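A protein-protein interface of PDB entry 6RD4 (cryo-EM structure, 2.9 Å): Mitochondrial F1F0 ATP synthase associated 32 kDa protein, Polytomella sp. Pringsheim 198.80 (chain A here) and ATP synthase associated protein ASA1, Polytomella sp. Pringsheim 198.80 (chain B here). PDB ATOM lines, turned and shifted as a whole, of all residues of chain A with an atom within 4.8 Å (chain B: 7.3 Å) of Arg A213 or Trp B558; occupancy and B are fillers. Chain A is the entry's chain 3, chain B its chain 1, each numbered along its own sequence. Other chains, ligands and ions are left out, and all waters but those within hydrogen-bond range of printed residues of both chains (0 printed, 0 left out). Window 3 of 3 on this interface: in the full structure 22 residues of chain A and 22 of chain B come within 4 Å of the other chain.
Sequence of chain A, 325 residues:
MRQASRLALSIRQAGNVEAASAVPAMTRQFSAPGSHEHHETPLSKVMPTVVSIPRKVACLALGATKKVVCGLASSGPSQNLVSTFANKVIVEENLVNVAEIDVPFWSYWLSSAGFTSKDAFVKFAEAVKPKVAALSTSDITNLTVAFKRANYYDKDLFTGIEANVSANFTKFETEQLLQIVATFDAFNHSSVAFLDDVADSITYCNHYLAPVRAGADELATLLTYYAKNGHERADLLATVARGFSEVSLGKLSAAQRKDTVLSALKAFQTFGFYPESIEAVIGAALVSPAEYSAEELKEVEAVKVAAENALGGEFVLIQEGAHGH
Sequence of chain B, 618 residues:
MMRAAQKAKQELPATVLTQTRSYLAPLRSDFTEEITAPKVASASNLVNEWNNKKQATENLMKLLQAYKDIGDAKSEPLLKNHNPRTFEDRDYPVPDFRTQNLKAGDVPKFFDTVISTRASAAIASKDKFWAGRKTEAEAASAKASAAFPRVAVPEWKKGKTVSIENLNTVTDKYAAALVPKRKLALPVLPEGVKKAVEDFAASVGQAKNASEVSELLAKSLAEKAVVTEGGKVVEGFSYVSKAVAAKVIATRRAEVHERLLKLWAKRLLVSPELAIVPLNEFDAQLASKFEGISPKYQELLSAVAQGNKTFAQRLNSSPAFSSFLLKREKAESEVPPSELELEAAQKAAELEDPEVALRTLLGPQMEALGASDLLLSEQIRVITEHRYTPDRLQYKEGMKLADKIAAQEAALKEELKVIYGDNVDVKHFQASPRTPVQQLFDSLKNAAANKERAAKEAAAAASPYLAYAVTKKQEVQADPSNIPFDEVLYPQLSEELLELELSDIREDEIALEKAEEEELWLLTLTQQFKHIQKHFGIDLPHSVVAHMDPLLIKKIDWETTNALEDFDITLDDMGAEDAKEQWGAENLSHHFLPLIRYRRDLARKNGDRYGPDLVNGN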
ATOM      1  N   HIS A 207      31.748  26.889 -18.205  1.00  0.00           N
ATOM      2  CA  HIS A 207      30.986  25.827 -17.574  1.00  0.00           C
ATOM      3  C   HIS A 207      31.898  24.687 -17.175  1.00  0.00           C
ATOM      4  O   HIS A 207      32.870  24.391 -17.857  1.00  0.00           O
ATOM      5  CB  HIS A 207      29.916  25.315 -18.513  1.00  0.00           C
ATOM      6  CG  HIS A 207      28.833  24.560 -17.821  1.00  0.00           C
ATOM      7  ND1 HIS A 207      28.933  23.227 -17.526  1.00  0.00           N
ATOM      8  CD2 HIS A 207      27.644  24.960 -17.335  1.00  0.00           C
ATOM      9  CE1 HIS A 207      27.846  22.831 -16.900  1.00  0.00           C
ATOM     10  NE2 HIS A 207      27.051  23.868 -16.765  1.00  0.00           N
ATOM     11  N   LEU A 209      31.536  21.557 -17.102  1.00  0.00           N
ATOM     12  CA  LEU A 209      31.494  20.388 -17.955  1.00  0.00           C
ATOM     13  C   LEU A 209      31.935  20.697 -19.356  1.00  0.00           C
ATOM     14  O   LEU A 209      31.776  19.859 -20.230  1.00  0.00           O
ATOM     15  CB  LEU A 209      30.095  19.808 -18.008  1.00  0.00           C
ATOM     16  CG  LEU A 209      29.398  19.447 -16.722  1.00  0.00           C
ATOM     17  CD1 LEU A 209      28.003  19.111 -17.063  1.00  0.00           C
ATOM     18  CD2 LEU A 209      30.065  18.285 -16.110  1.00  0.00           C
ATOM     19  N   ALA A 210      32.434  21.866 -19.602  1.00  0.00           N
ATOM     20  CA  ALA A 210      33.039  22.153 -20.887  1.00  0.00           C
ATOM     21  C   ALA A 210      34.303  21.347 -21.189  1.00  0.00           C
ATOM     22  O   ALA A 210      34.593  21.157 -22.371  1.00  0.00           O
ATOM     23  CB  ALA A 210      33.333  23.641 -21.006  1.00  0.00           C
ATOM     24  N   PRO A 211      35.101  20.882 -20.215  1.00  0.00           N
ATOM     25  CA  PRO A 211      36.098  19.864 -20.555  1.00  0.00           C
ATOM     26  C   PRO A 211      35.534  18.538 -21.008  1.00  0.00           C
ATOM     27  O   PRO A 211      36.209  17.816 -21.742  1.00  0.00           O
ATOM     28  CB  PRO A 211      36.859  19.713 -19.246  1.00  0.00           C
ATOM     29  CG  PRO A 211      36.854  21.000 -18.726  1.00  0.00           C
ATOM     30  CD  PRO A 211      35.537  21.557 -18.976  1.00  0.00           C
ATOM     31  N   VAL A 212      34.329  18.180 -20.584  1.00  0.00           N
ATOM     32  CA  VAL A 212      33.742  16.903 -20.963  1.00  0.00           C
ATOM     33  C   VAL A 212      33.355  16.899 -22.436  1.00  0.00           C
ATOM     34  O   VAL A 212      33.356  15.852 -23.088  1.00  0.00           O
ATOM     35  CB  VAL A 212      32.562  16.640 -20.022  1.00  0.00           C
ATOM     36  CG1 VAL A 212      31.944  15.351 -20.283  1.00  0.00           C
ATOM     37  CG2 VAL A 212      33.046  16.648 -18.620  1.00  0.00           C
ATOM     38  N   ARG A 213      33.073  18.060 -22.997  1.00  0.00           N
ATOM     39  CA  ARG A 213      32.754  18.215 -24.402  1.00  0.00           C
ATOM     40  C   ARG A 213      33.966  18.464 -25.269  1.00  0.00           C
ATOM     41  O   ARG A 213      33.805  18.893 -26.409  1.00  0.00           O
ATOM     42  CB  ARG A 213      31.787  19.376 -24.584  1.00  0.00           C
ATOM     43  CG  ARG A 213      30.367  19.045 -24.279  1.00  0.00           C
ATOM     44  CD  ARG A 213      29.689  18.497 -25.496  1.00  0.00           C
ATOM     45  NE  ARG A 213      28.271  18.380 -25.266  1.00  0.00           N
ATOM     46  CZ  ARG A 213      27.706  17.328 -24.707  1.00  0.00           C
ATOM     47  NH1 ARG A 213      26.405  17.303 -24.511  1.00  0.00           N
ATOM     48  NH2 ARG A 213      28.444  16.292 -24.357  1.00  0.00           N
ATOM     49  N   ALA A 214      35.170  18.218 -24.777  1.00  0.00           N
ATOM     50  CA  ALA A 214      36.358  18.728 -25.447  1.00  0.00           C
ATOM     51  C   ALA A 214      37.065  17.700 -26.306  1.00  0.00           C
ATOM     52  O   ALA A 214      37.554  18.035 -27.385  1.00  0.00           O
ATOM     53  CB  ALA A 214      37.350  19.275 -24.427  1.00  0.00           C
ATOM     54  N   GLY A 215      37.154  16.465 -25.857  1.00  0.00           N
ATOM     55  CA  GLY A 215      37.955  15.514 -26.593  1.00  0.00           C
ATOM     56  C   GLY A 215      39.358  15.537 -26.049  1.00  0.00           C
ATOM     57  O   GLY A 215      40.009  16.580 -26.043  1.00  0.00           O
ATOM     58  N   LEU B 552      27.103  34.033 -15.342  1.00  0.00           N
ATOM     59  CA  LEU B 552      26.128  33.025 -14.966  1.00  0.00           C
ATOM     60  C   LEU B 552      25.226  32.719 -16.131  1.00  0.00           C
ATOM     61  O   LEU B 552      24.914  31.563 -16.394  1.00  0.00           O
ATOM     62  CB  LEU B 552      25.297  33.491 -13.787  1.00  0.00           C
ATOM     63  CG  LEU B 552      24.227  32.527 -13.329  1.00  0.00           C
ATOM     64  CD1 LEU B 552      24.840  31.288 -12.816  1.00  0.00           C
ATOM     65  CD2 LEU B 552      23.393  33.132 -12.299  1.00  0.00           C
ATOM     66  N   ILE B 553      24.817  33.753 -16.851  1.00  0.00           N
ATOM     67  CA  ILE B 553      24.048  33.607 -18.071  1.00  0.00           C
ATOM     68  C   ILE B 553      24.864  32.917 -19.144  1.00  0.00           C
ATOM     69  O   ILE B 553      24.332  32.120 -19.904  1.00  0.00           O
ATOM     70  CB  ILE B 553      23.570  35.004 -18.483  1.00  0.00           C
ATOM     71  CG1 ILE B 553      22.600  35.536 -17.445  1.00  0.00           C
ATOM     72  CG2 ILE B 553      22.976  35.032 -19.818  1.00  0.00           C
ATOM     73  CD1 ILE B 553      21.468  34.651 -17.157  1.00  0.00           C
ATOM     74  N   LYS B 554      26.167  33.157 -19.188  1.00  0.00           N
ATOM     75  CA  LYS B 554      27.043  32.506 -20.151  1.00  0.00           C
ATOM     76  C   LYS B 554      27.146  31.015 -19.901  1.00  0.00           C
ATOM     77  O   LYS B 554      27.181  30.230 -20.843  1.00  0.00           O
ATOM     78  CB  LYS B 554      28.423  33.132 -20.089  1.00  0.00           C
ATOM     79  CG  LYS B 554      29.386  32.624 -21.099  1.00  0.00           C
ATOM     80  CD  LYS B 554      30.771  32.771 -20.612  1.00  0.00           C
ATOM     81  CE  LYS B 554      31.735  32.259 -21.599  1.00  0.00           C
ATOM     82  NZ  LYS B 554      33.074  32.223 -20.999  1.00  0.00           N
ATOM     83  N   LYS B 555      27.194  30.604 -18.643  1.00  0.00           N
ATOM     84  CA  LYS B 555      27.277  29.193 -18.314  1.00  0.00           C
ATOM     85  C   LYS B 555      25.934  28.501 -18.376  1.00  0.00           C
ATOM     86  O   LYS B 555      25.887  27.297 -18.584  1.00  0.00           O
ATOM     87  CB  LYS B 555      27.841  29.015 -16.922  1.00  0.00           C
ATOM     88  CG  LYS B 555      29.232  29.440 -16.766  1.00  0.00           C
ATOM     89  CD  LYS B 555      29.672  29.183 -15.390  1.00  0.00           C
ATOM     90  CE  LYS B 555      30.514  30.268 -14.906  1.00  0.00           C
ATOM     91  NZ  LYS B 555      31.294  29.806 -13.776  1.00  0.00           N
ATOM     92  N   ILE B 556      24.845  29.216 -18.124  1.00  0.00           N
ATOM     93  CA  ILE B 556      23.511  28.668 -18.321  1.00  0.00           C
ATOM     94  C   ILE B 556      23.258  28.419 -19.793  1.00  0.00           C
ATOM     95  O   ILE B 556      22.735  27.374 -20.176  1.00  0.00           O
ATOM     96  CB  ILE B 556      22.466  29.615 -17.717  1.00  0.00           C
ATOM     97  CG1 ILE B 556      22.392  29.458 -16.215  1.00  0.00           C
ATOM     98  CG2 ILE B 556      21.136  29.360 -18.260  1.00  0.00           C
ATOM     99  CD1 ILE B 556      21.680  30.557 -15.585  1.00  0.00           C
ATOM    100  N   ASP B 557      23.667  29.353 -20.643  1.00  0.00           N
ATOM    101  CA  ASP B 557      23.543  29.197 -22.080  1.00  0.00           C
ATOM    102  C   ASP B 557      24.413  28.098 -22.632  1.00  0.00           C
ATOM    103  O   ASP B 557      24.171  27.653 -23.744  1.00  0.00           O
ATOM    104  CB  ASP B 557      23.927  30.476 -22.790  1.00  0.00           C
ATOM    105  CG  ASP B 557      22.938  31.554 -22.601  1.00  0.00           C
ATOM    106  OD1 ASP B 557      21.962  31.333 -21.880  1.00  0.00           O
ATOM    107  OD2 ASP B 557      23.131  32.629 -23.182  1.00  0.00           O
ATOM    108  N   TRP B 558      25.454  27.695 -21.927  1.00  0.00           N
ATOM    109  CA  TRP B 558      26.244  26.572 -22.395  1.00  0.00           C
ATOM    110  C   TRP B 558      25.480  25.279 -22.241  1.00  0.00           C
ATOM    111  O   TRP B 558      25.633  24.372 -23.049  1.00  0.00           O
ATOM    112  CB  TRP B 558      27.569  26.495 -21.652  1.00  0.00           C
ATOM    113  CG  TRP B 558      28.470  25.450 -22.177  1.00  0.00           C
ATOM    114  CD1 TRP B 558      29.391  25.597 -23.130  1.00  0.00           C
ATOM    115  CD2 TRP B 558      28.520  24.082 -21.774  1.00  0.00           C
ATOM    116  NE1 TRP B 558      30.018  24.414 -23.362  1.00  0.00           N
ATOM    117  CE2 TRP B 558      29.495  23.472 -22.526  1.00  0.00           C
ATOM    118  CE3 TRP B 558      27.826  23.321 -20.845  1.00  0.00           C
ATOM    119  CZ2 TRP B 558      29.779  22.149 -22.403  1.00  0.00           C
ATOM    120  CZ3 TRP B 558      28.107  22.034 -20.725  1.00  0.00           C
ATOM    121  CH2 TRP B 558      29.071  21.447 -21.488  1.00  0.00           C
ATOM    122  N   GLU B 559      24.671  25.162 -21.203  1.00  0.00           N
ATOM    123  CA  GLU B 559      23.895  23.951 -21.025  1.00  0.00           C
ATOM    124  C   GLU B 559      22.781  23.855 -22.044  1.00  0.00           C
ATOM    125  O   GLU B 559      22.441  22.762 -22.483  1.00  0.00           O
ATOM    126  CB  GLU B 559      23.322  23.915 -19.633  1.00  0.00           C
ATOM    127  CG  GLU B 559      24.311  24.173 -18.602  1.00  0.00           C
ATOM    128  CD  GLU B 559      23.824  23.784 -17.259  1.00  0.00           C
ATOM    129  OE1 GLU B 559      22.861  23.019 -17.191  1.00  0.00           O
ATOM    130  OE2 GLU B 559      24.389  24.243 -16.263  1.00  0.00           O
ATOM    131  N   THR B 560      22.178  24.974 -22.412  1.00  0.00           N
ATOM    132  CA  THR B 560      21.151  24.934 -23.438  1.00  0.00           C
ATOM    133  C   THR B 560      21.756  24.654 -24.798  1.00  0.00           C
ATOM    134  O   THR B 560      21.176  23.921 -25.589  1.00  0.00           O
ATOM    135  CB  THR B 560      20.373  26.238 -23.456  1.00  0.00           C
ATOM    136  OG1 THR B 560      19.999  26.573 -22.125  1.00  0.00           O
ATOM    137  CG2 THR B 560      19.144  26.096 -24.236  1.00  0.00           C
ATOM    138  N   THR B 561      22.930  25.207 -25.073  1.00  0.00           N
ATOM    139  CA  THR B 561      23.570  24.989 -26.362  1.00  0.00           C
ATOM    140  C   THR B 561      24.031  23.559 -26.508  1.00  0.00           C
ATOM    141  O   THR B 561      23.862  22.946 -27.560  1.00  0.00           O
ATOM    142  CB  THR B 561      24.742  25.933 -26.509  1.00  0.00           C
ATOM    143  OG1 THR B 561      24.282  27.266 -26.338  1.00  0.00           O
ATOM    144  CG2 THR B 561      25.352  25.823 -27.842  1.00  0.00           C
ATOM    145  N   ASN B 562      24.573  22.997 -25.443  1.00  0.00           N
ATOM    146  CA  ASN B 562      25.123  21.657 -25.459  1.00  0.00           C
ATOM    147  C   ASN B 562      24.172  20.639 -24.899  1.00  0.00           C
ATOM    148  O   ASN B 562      24.609  19.702 -24.241  1.00  0.00           O
ATOM    149  CB  ASN B 562      26.428  21.638 -24.702  1.00  0.00           C
ATOM    150  CG  ASN B 562      27.442  22.457 -25.370  1.00  0.00           C
ATOM    151  OD1 ASN B 562      27.494  23.646 -25.177  1.00  0.00           O
ATOM    152  ND2 ASN B 562      28.227  21.847 -26.216  1.00  0.00           N
ATOM    153  N   ALA B 563      22.881  20.857 -25.100  1.00  0.00           N
ATOM    154  CA  ALA B 563      21.821  19.873 -24.956  1.00  0.00           C
ATOM    155  C   ALA B 563      21.700  19.323 -23.557  1.00  0.00           C
ATOM    156  O   ALA B 563      21.220  18.212 -23.368  1.00  0.00           O
ATOM    157  CB  ALA B 563      22.004  18.732 -25.946  1.00  0.00           C
ATOM    158  N   LEU B 564      22.144  20.067 -22.565  1.00  0.00           N
ATOM    159  CA  LEU B 564      22.041  19.674 -21.176  1.00  0.00           C
ATOM    160  C   LEU B 564      21.133  20.624 -20.428  1.00  0.00           C
ATOM    161  O   LEU B 564      21.383  20.951 -19.279  1.00  0.00           O
ATOM    162  CB  LEU B 564      23.400  19.659 -20.503  1.00  0.00           C
ATOM    163  CG  LEU B 564      24.542  18.807 -21.003  1.00  0.00           C
ATOM    164  CD1 LEU B 564      25.768  19.355 -20.401  1.00  0.00           C
ATOM    165  CD2 LEU B 564      24.349  17.419 -20.542  1.00  0.00           C
ATOM    166  N   GLU B 565      20.061  21.079 -21.071  1.00  0.00           N
ATOM    167  CA  GLU B 565      19.166  22.022 -20.424  1.00  0.00           C
ATOM    168  C   GLU B 565      18.361  21.388 -19.311  1.00  0.00           C
ATOM    169  O   GLU B 565      17.713  22.099 -18.549  1.00  0.00           O
ATOM    170  CB  GLU B 565      18.217  22.652 -21.433  1.00  0.00           C
ATOM    171  CG  GLU B 565      17.214  21.707 -21.993  1.00  0.00           C
ATOM    172  CD  GLU B 565      17.659  21.097 -23.281  1.00  0.00           C
ATOM    173  OE1 GLU B 565      18.812  21.328 -23.671  1.00  0.00           O
ATOM    174  OE2 GLU B 565      16.872  20.368 -23.905  1.00  0.00           O
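Arg A213 touches just these residues of chain B: Trp B558 (3.7 Å) and Asn B562 (3.0 Å).
Of chain A, only His A207, Leu A209, Ala A210 and Arg A213 come within 4 Å of Trp B558.
Of the printed residues of chain B, His A207 touches Lys B555, Trp B558 and Glu B559.
Printed residues of chain A within 4 Å of Asn B562: Arg A213 (3.0 Å).
Asp B557 touches none of the printed residues of chain A.
Gly A215 touches none of the printed residues of chain B.
The nearest printed residue of chain B that does not touch His A207 is Ile B556 (5.2 Å).
Among the printed residues, merely in contact across the chains: His A207 with Lys B555 (3.2 Å), Leu A209 with Trp B558 (3.4 Å), His A207 with Trp B558 (3.4 Å), Ala A210 with Trp B558 (3.6 Å) and Arg A213 with Trp B558 (3.7 Å).
O of Glu B559 is in hydrogen-bond range of N of Glu B565, at 3.2 Å.
The backbone carbonyl oxygen (O) of Trp B558 sits close to the side-chain amide oxygen (OD1) of Asn B562 (2.9 Å).
The backbone NH (N) of Leu A209 is in hydrogen-bond range of a ring nitrogen (ND1) of His A207, 3.1 Å away.
The backbone NH of Leu B564 sits at hydrogen-bond distance from the backbone carbonyl oxygen of Glu B559 (2.7 Å).
Hydrophobic or aromatic side chains of chain B that line the printed part of chain A: Trp B558.
Along chain B the printed residues that touch a printed residue of chain A span positions 555 to 562.
Of the 8 printed residues of chain A, 4 touch a printed residue of chain B.
Printed residues of chain A that touch a printed residue of chain B: His A207, Leu A209, Ala A210 and Arg A213.
Hydrophobic or aromatic side chains of chain A within 4 Å of the printed part of chain B: His A207 and Leu A209.
Among the printed residues, 7 pairs touch across the chains.
Among the printed residues, no Asp or Glu carboxylate lies within 4 Å of a Lys or Arg side-chain nitrogen of the other chain.
O of Asn B562 is in hydrogen-bond range of NH1 of Arg A213, 3.0 Å away.
NE2 of His A207 lies within hydrogen-bond range of OE2 of Glu B559 (2.7 Å).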
